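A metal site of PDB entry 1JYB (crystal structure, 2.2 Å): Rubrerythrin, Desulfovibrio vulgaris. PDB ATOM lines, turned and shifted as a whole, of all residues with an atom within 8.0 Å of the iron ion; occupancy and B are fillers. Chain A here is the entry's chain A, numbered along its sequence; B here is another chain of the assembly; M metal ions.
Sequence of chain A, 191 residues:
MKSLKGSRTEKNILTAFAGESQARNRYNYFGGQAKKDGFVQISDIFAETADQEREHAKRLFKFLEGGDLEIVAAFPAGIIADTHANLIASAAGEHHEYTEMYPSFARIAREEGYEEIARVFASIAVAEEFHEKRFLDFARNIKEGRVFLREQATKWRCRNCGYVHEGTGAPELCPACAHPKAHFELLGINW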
ATOM      1  N   ARG A 157      -9.263  -7.045  29.363  1.00  0.00           N
ATOM      2  CA  ARG A 157      -9.857  -7.935  28.373  1.00  0.00           C
ATOM      3  C   ARG A 157     -10.331  -7.150  27.144  1.00  0.00           C
ATOM      4  O   ARG A 157     -10.953  -6.099  27.287  1.00  0.00           O
ATOM      5  CB  ARG A 157     -11.049  -8.663  28.931  1.00  0.00           C
ATOM      6  CG  ARG A 157     -11.405  -9.854  28.082  1.00  0.00           C
ATOM      7  CD  ARG A 157     -12.618 -10.574  28.561  1.00  0.00           C
ATOM      8  NE  ARG A 157     -13.724  -9.623  28.497  1.00  0.00           N
ATOM      9  CZ  ARG A 157     -14.902  -9.921  27.937  1.00  0.00           C
ATOM     10  NH1 ARG A 157     -15.134 -11.103  27.410  1.00  0.00           N
ATOM     11  NH2 ARG A 157     -15.855  -9.004  27.817  1.00  0.00           N
ATOM     12  N   CYS A 158     -10.018  -7.646  25.960  1.00  0.00           N
ATOM     13  CA  CYS A 158     -10.511  -7.172  24.687  1.00  0.00           C
ATOM     14  C   CYS A 158     -11.908  -7.702  24.573  1.00  0.00           C
ATOM     15  O   CYS A 158     -12.102  -8.922  24.509  1.00  0.00           O
ATOM     16  CB  CYS A 158      -9.743  -7.731  23.559  1.00  0.00           C
ATOM     17  SG  CYS A 158     -10.234  -7.220  21.892  1.00  0.00           S
ATOM     18  N   ARG A 159     -12.840  -6.772  24.487  1.00  0.00           N
ATOM     19  CA  ARG A 159     -14.218  -7.120  24.321  1.00  0.00           C
ATOM     20  C   ARG A 159     -14.479  -7.666  22.938  1.00  0.00           C
ATOM     21  O   ARG A 159     -15.459  -8.400  22.724  1.00  0.00           O
ATOM     22  CB  ARG A 159     -15.103  -5.941  24.517  1.00  0.00           C
ATOM     23  CG  ARG A 159     -14.950  -5.365  25.894  1.00  0.00           C
ATOM     24  CD  ARG A 159     -15.807  -4.125  26.029  1.00  0.00           C
ATOM     25  NE  ARG A 159     -17.064  -4.536  26.625  1.00  0.00           N
ATOM     26  CZ  ARG A 159     -18.150  -4.730  25.898  1.00  0.00           C
ATOM     27  NH1 ARG A 159     -18.127  -4.553  24.569  1.00  0.00           N
ATOM     28  NH2 ARG A 159     -19.266  -5.138  26.481  1.00  0.00           N
ATOM     29  N   ASN A 160     -13.642  -7.320  21.960  1.00  0.00           N
ATOM     30  CA  ASN A 160     -13.868  -7.853  20.662  1.00  0.00           C
ATOM     31  C   ASN A 160     -13.409  -9.310  20.567  1.00  0.00           C
ATOM     32  O   ASN A 160     -14.204 -10.119  20.091  1.00  0.00           O
ATOM     33  CB  ASN A 160     -13.150  -7.023  19.676  1.00  0.00           C
ATOM     34  CG  ASN A 160     -13.622  -7.326  18.262  1.00  0.00           C
ATOM     35  OD1 ASN A 160     -12.821  -7.594  17.355  1.00  0.00           O
ATOM     36  ND2 ASN A 160     -14.896  -7.181  17.934  1.00  0.00           N
ATOM     37  N   CYS A 161     -12.249  -9.770  21.056  1.00  0.00           N
ATOM     38  CA  CYS A 161     -11.908 -11.162  20.835  1.00  0.00           C
ATOM     39  C   CYS A 161     -11.624 -11.946  22.105  1.00  0.00           C
ATOM     40  O   CYS A 161     -11.363 -13.159  22.030  1.00  0.00           O
ATOM     41  CB  CYS A 161     -10.705 -11.269  19.931  1.00  0.00           C
ATOM     42  SG  CYS A 161      -9.199 -10.694  20.783  1.00  0.00           S
ATOM     43  N   GLY A 162     -11.645 -11.296  23.274  1.00  0.00           N
ATOM     44  CA  GLY A 162     -11.462 -11.937  24.561  1.00  0.00           C
ATOM     45  C   GLY A 162     -10.027 -12.143  24.989  1.00  0.00           C
ATOM     46  O   GLY A 162      -9.771 -12.858  25.977  1.00  0.00           O
ATOM     47  N   TYR A 163      -9.077 -11.547  24.278  1.00  0.00           N
ATOM     48  CA  TYR A 163      -7.695 -11.615  24.637  1.00  0.00           C
ATOM     49  C   TYR A 163      -7.475 -10.994  26.024  1.00  0.00           C
ATOM     50  O   TYR A 163      -8.014  -9.919  26.304  1.00  0.00           O
ATOM     51  CB  TYR A 163      -6.888 -10.885  23.550  1.00  0.00           C
ATOM     52  CG  TYR A 163      -5.396 -10.792  23.850  1.00  0.00           C
ATOM     53  CD1 TYR A 163      -4.582 -11.901  23.733  1.00  0.00           C
ATOM     54  CD2 TYR A 163      -4.887  -9.605  24.343  1.00  0.00           C
ATOM     55  CE1 TYR A 163      -3.227 -11.818  24.067  1.00  0.00           C
ATOM     56  CE2 TYR A 163      -3.544  -9.514  24.696  1.00  0.00           C
ATOM     57  CZ  TYR A 163      -2.730 -10.630  24.567  1.00  0.00           C
ATOM     58  OH  TYR A 163      -1.404 -10.510  24.860  1.00  0.00           O
ATOM     59  N   VAL A 164      -6.752 -11.676  26.935  1.00  0.00           N
ATOM     60  CA  VAL A 164      -6.469 -11.091  28.237  1.00  0.00           C
ATOM     61  C   VAL A 164      -5.017 -10.616  28.271  1.00  0.00           C
ATOM     62  O   VAL A 164      -4.084 -11.291  27.831  1.00  0.00           O
ATOM     63  CB  VAL A 164      -6.755 -12.123  29.345  1.00  0.00           C
ATOM     64  CG1 VAL A 164      -6.386 -11.536  30.724  1.00  0.00           C
ATOM     65  CG2 VAL A 164      -8.238 -12.497  29.298  1.00  0.00           C
ATOM     66  N   LEU A 173      -3.106  -1.901  20.354  1.00  0.00           N
ATOM     67  CA  LEU A 173      -3.852  -2.722  19.432  1.00  0.00           C
ATOM     68  C   LEU A 173      -3.900  -4.063  20.067  1.00  0.00           C
ATOM     69  O   LEU A 173      -2.879  -4.484  20.592  1.00  0.00           O
ATOM     70  CB  LEU A 173      -3.156  -2.909  18.126  1.00  0.00           C
ATOM     71  CG  LEU A 173      -3.131  -1.747  17.185  1.00  0.00           C
ATOM     72  CD1 LEU A 173      -2.372  -2.165  15.963  1.00  0.00           C
ATOM     73  CD2 LEU A 173      -4.523  -1.346  16.773  1.00  0.00           C
ATOM     74  N   CYS A 174      -5.004  -4.736  20.066  1.00  0.00           N
ATOM     75  CA  CYS A 174      -5.038  -6.066  20.555  1.00  0.00           C
ATOM     76  C   CYS A 174      -4.159  -7.007  19.686  1.00  0.00           C
ATOM     77  O   CYS A 174      -4.326  -7.068  18.460  1.00  0.00           O
ATOM     78  CB  CYS A 174      -6.462  -6.473  20.530  1.00  0.00           C
ATOM     79  SG  CYS A 174      -6.697  -8.200  20.961  1.00  0.00           S
ATOM     80  N   PRO A 175      -3.212  -7.804  20.196  1.00  0.00           N
ATOM     81  CA  PRO A 175      -2.432  -8.722  19.351  1.00  0.00           C
ATOM     82  C   PRO A 175      -3.169  -9.894  18.691  1.00  0.00           C
ATOM     83  O   PRO A 175      -2.660 -10.466  17.726  1.00  0.00           O
ATOM     84  CB  PRO A 175      -1.342  -9.127  20.300  1.00  0.00           C
ATOM     85  CG  PRO A 175      -1.966  -9.072  21.664  1.00  0.00           C
ATOM     86  CD  PRO A 175      -2.775  -7.811  21.598  1.00  0.00           C
ATOM     87  N   ALA A 176      -4.327 -10.306  19.217  1.00  0.00           N
ATOM     88  CA  ALA A 176      -5.078 -11.397  18.649  1.00  0.00           C
ATOM     89  C   ALA A 176      -5.984 -10.881  17.549  1.00  0.00           C
ATOM     90  O   ALA A 176      -5.935 -11.454  16.459  1.00  0.00           O
ATOM     91  CB  ALA A 176      -5.945 -12.051  19.704  1.00  0.00           C
ATOM     92  N   CYS A 177      -6.805  -9.814  17.716  1.00  0.00           N
ATOM     93  CA  CYS A 177      -7.770  -9.377  16.695  1.00  0.00           C
ATOM     94  C   CYS A 177      -7.357  -8.093  16.018  1.00  0.00           C
ATOM     95  O   CYS A 177      -8.040  -7.641  15.099  1.00  0.00           O
ATOM     96  CB  CYS A 177      -9.199  -9.129  17.250  1.00  0.00           C
ATOM     97  SG  CYS A 177      -9.324  -7.719  18.410  1.00  0.00           S
ATOM     98  N   ALA A 178      -6.259  -7.463  16.450  1.00  0.00           N
ATOM     99  CA  ALA A 178      -5.745  -6.185  15.945  1.00  0.00           C
ATOM    100  C   ALA A 178      -6.741  -5.035  15.997  1.00  0.00           C
ATOM    101  O   ALA A 178      -6.721  -4.141  15.144  1.00  0.00           O
ATOM    102  CB  ALA A 178      -5.252  -6.301  14.506  1.00  0.00           C
ATOM    103  N   HIS A 179      -7.681  -5.018  16.942  1.00  0.00           N
ATOM    104  CA  HIS A 179      -8.582  -3.881  17.088  1.00  0.00           C
ATOM    105  C   HIS A 179      -7.938  -2.973  18.119  1.00  0.00           C
ATOM    106  O   HIS A 179      -7.091  -3.404  18.908  1.00  0.00           O
ATOM    107  CB  HIS A 179      -9.978  -4.367  17.542  1.00  0.00           C
ATOM    108  CG  HIS A 179     -10.799  -4.972  16.404  1.00  0.00           C
ATOM    109  ND1 HIS A 179     -10.441  -5.907  15.528  1.00  0.00           N
ATOM    110  CD2 HIS A 179     -12.080  -4.599  16.088  1.00  0.00           C
ATOM    111  CE1 HIS A 179     -11.425  -6.104  14.683  1.00  0.00           C
ATOM    112  NE2 HIS A 179     -12.411  -5.312  15.042  1.00  0.00           N
ATOM    113  N   PRO A 180      -8.197  -1.669  18.114  1.00  0.00           N
ATOM    114  CA  PRO A 180      -7.463  -0.756  18.988  1.00  0.00           C
ATOM    115  C   PRO A 180      -7.908  -0.770  20.443  1.00  0.00           C
ATOM    116  O   PRO A 180      -8.939  -1.351  20.819  1.00  0.00           O
ATOM    117  CB  PRO A 180      -7.632   0.603  18.318  1.00  0.00           C
ATOM    118  CG  PRO A 180      -8.943   0.454  17.621  1.00  0.00           C
ATOM    119  CD  PRO A 180      -8.801  -0.935  17.019  1.00  0.00           C
ATOM    120  N   HIS A 183     -11.283  -1.091  22.571  1.00  0.00           N
ATOM    121  CA  HIS A 183     -11.986  -2.344  22.862  1.00  0.00           C
ATOM    122  C   HIS A 183     -11.817  -3.040  24.190  1.00  0.00           C
ATOM    123  O   HIS A 183     -12.606  -3.938  24.520  1.00  0.00           O
ATOM    124  CB  HIS A 183     -11.662  -3.349  21.829  1.00  0.00           C
ATOM    125  CG  HIS A 183     -12.413  -2.918  20.614  1.00  0.00           C
ATOM    126  ND1 HIS A 183     -13.629  -3.324  20.258  1.00  0.00           N
ATOM    127  CD2 HIS A 183     -11.973  -1.987  19.713  1.00  0.00           C
ATOM    128  CE1 HIS A 183     -13.962  -2.675  19.175  1.00  0.00           C
ATOM    129  NE2 HIS A 183     -12.959  -1.880  18.833  1.00  0.00           N
ATOM    130  N   PHE A 184     -10.828  -2.582  24.936  1.00  0.00           N
ATOM    131  CA  PHE A 184     -10.440  -3.154  26.198  1.00  0.00           C
ATOM    132  C   PHE A 184     -11.230  -2.635  27.407  1.00  0.00           C
ATOM    133  O   PHE A 184     -11.673  -1.478  27.517  1.00  0.00           O
ATOM    134  CB  PHE A 184      -8.939  -2.902  26.335  1.00  0.00           C
ATOM    135  CG  PHE A 184      -8.040  -3.891  25.604  1.00  0.00           C
ATOM    136  CD1 PHE A 184      -7.592  -3.640  24.329  1.00  0.00           C
ATOM    137  CD2 PHE A 184      -7.722  -5.113  26.214  1.00  0.00           C
ATOM    138  CE1 PHE A 184      -6.836  -4.595  23.671  1.00  0.00           C
ATOM    139  CE2 PHE A 184      -6.961  -6.076  25.552  1.00  0.00           C
ATOM    140  CZ  PHE A 184      -6.529  -5.810  24.276  1.00  0.00           C
ATOM    141  N   GLN B  52     -16.916 -13.820  19.708  1.00  0.00           N
ATOM    142  CA  GLN B  52     -15.486 -13.655  19.780  1.00  0.00           C
ATOM    143  C   GLN B  52     -14.873 -14.668  18.845  1.00  0.00           C
ATOM    144  O   GLN B  52     -13.870 -14.337  18.222  1.00  0.00           O
ATOM    145  CB  GLN B  52     -15.044 -13.860  21.219  1.00  0.00           C
ATOM    146  CG  GLN B  52     -15.583 -12.622  21.979  1.00  0.00           C
ATOM    147  CD  GLN B  52     -15.217 -12.651  23.457  1.00  0.00           C
ATOM    148  OE1 GLN B  52     -15.030 -13.735  24.020  1.00  0.00           O
ATOM    149  NE2 GLN B  52     -15.053 -11.526  24.115  1.00  0.00           N
ATOM    150  N   GLU B  55     -14.515 -13.305  15.490  1.00  0.00           N
ATOM    151  CA  GLU B  55     -13.390 -12.424  15.300  1.00  0.00           C
ATOM    152  C   GLU B  55     -12.024 -13.037  15.210  1.00  0.00           C
ATOM    153  O   GLU B  55     -11.120 -12.536  14.546  1.00  0.00           O
ATOM    154  CB  GLU B  55     -13.417 -11.392  16.402  1.00  0.00           C
ATOM    155  CG  GLU B  55     -14.655 -10.502  16.263  1.00  0.00           C
ATOM    156  CD  GLU B  55     -14.823  -9.663  14.973  1.00  0.00           C
ATOM    157  OE1 GLU B  55     -13.882  -8.955  14.607  1.00  0.00           O
ATOM    158  OE2 GLU B  55     -15.894  -9.688  14.359  1.00  0.00           O
ATOM    159  N   HIS B  56     -11.828 -14.135  15.873  1.00  0.00           N
ATOM    160  CA  HIS B  56     -10.582 -14.852  15.735  1.00  0.00           C
ATOM    161  C   HIS B  56     -10.557 -15.435  14.311  1.00  0.00           C
ATOM    162  O   HIS B  56      -9.539 -15.426  13.634  1.00  0.00           O
ATOM    163  CB  HIS B  56     -10.518 -16.020  16.716  1.00  0.00           C
ATOM    164  CG  HIS B  56     -10.448 -15.656  18.193  1.00  0.00           C
ATOM    165  ND1 HIS B  56     -10.889 -16.401  19.205  1.00  0.00           N
ATOM    166  CD2 HIS B  56      -9.923 -14.505  18.733  1.00  0.00           C
ATOM    167  CE1 HIS B  56     -10.651 -15.765  20.326  1.00  0.00           C
ATOM    168  NE2 HIS B  56     -10.066 -14.631  20.019  1.00  0.00           N
ATOM    169  N   SER B 123      -1.458 -15.465  20.412  1.00  0.00           N
ATOM    170  CA  SER B 123      -2.352 -14.541  21.092  1.00  0.00           C
ATOM    171  C   SER B 123      -3.795 -15.008  21.169  1.00  0.00           C
ATOM    172  O   SER B 123      -4.464 -14.799  22.182  1.00  0.00           O
ATOM    173  CB  SER B 123      -2.299 -13.207  20.396  1.00  0.00           C
ATOM    174  OG  SER B 123      -1.024 -12.610  20.573  1.00  0.00           O
ATOM    175  N   ALA B 127      -6.905 -15.981  24.768  1.00  0.00           N
ATOM    176  CA  ALA B 127      -8.350 -15.817  24.762  1.00  0.00           C
ATOM    177  C   ALA B 127      -9.024 -17.153  24.905  1.00  0.00           C
ATOM    178  O   ALA B 127     -10.060 -17.282  25.555  1.00  0.00           O
ATOM    179  CB  ALA B 127      -8.769 -15.187  23.439  1.00  0.00           C
HETATM  180 FE    FE M   1      -8.919  -8.464  20.538  1.00  0.00          FE
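The iron ion is bound by SG of Cys 161 (2.3 Å). SG of Cys 158 is bound to the iron ion, 2.3 Å away. SG of Cys 174 binds the iron ion (2.3 Å). The iron ion is bound by SG of Cys 177. The iron ion has four donor atoms within binding distance.
Within 4 Å of the iron ion: Cys 158, Cys 161, Cys 174 and Cys 177.
The backbone carbonyl oxygen (O) of Cys 161 lies within hydrogen-bond range of a ring nitrogen (NE2) of His 56 of chain B, 2.8 Å away. N of Cys 158 sits at hydrogen-bond distance from O of Tyr 163, 3.0 Å away. N of Asn 160 sits close to SG of Cys 158 (3.4 Å). The side-chain sulfur of Cys 161 lies close to the backbone NH of Tyr 163 (3.6 Å). ND1 of His 179 is in hydrogen-bond range of O of Cys 177 (3.0 Å). The backbone NH (N) of Ala 176 lies close to the side-chain sulfur (SG) of Cys 174 (3.6 Å). SG of Cys 177 sits close to OD1 of Asn 160 (3.7 Å). O of His 179 lies within hydrogen-bond range of N of Cys 174.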
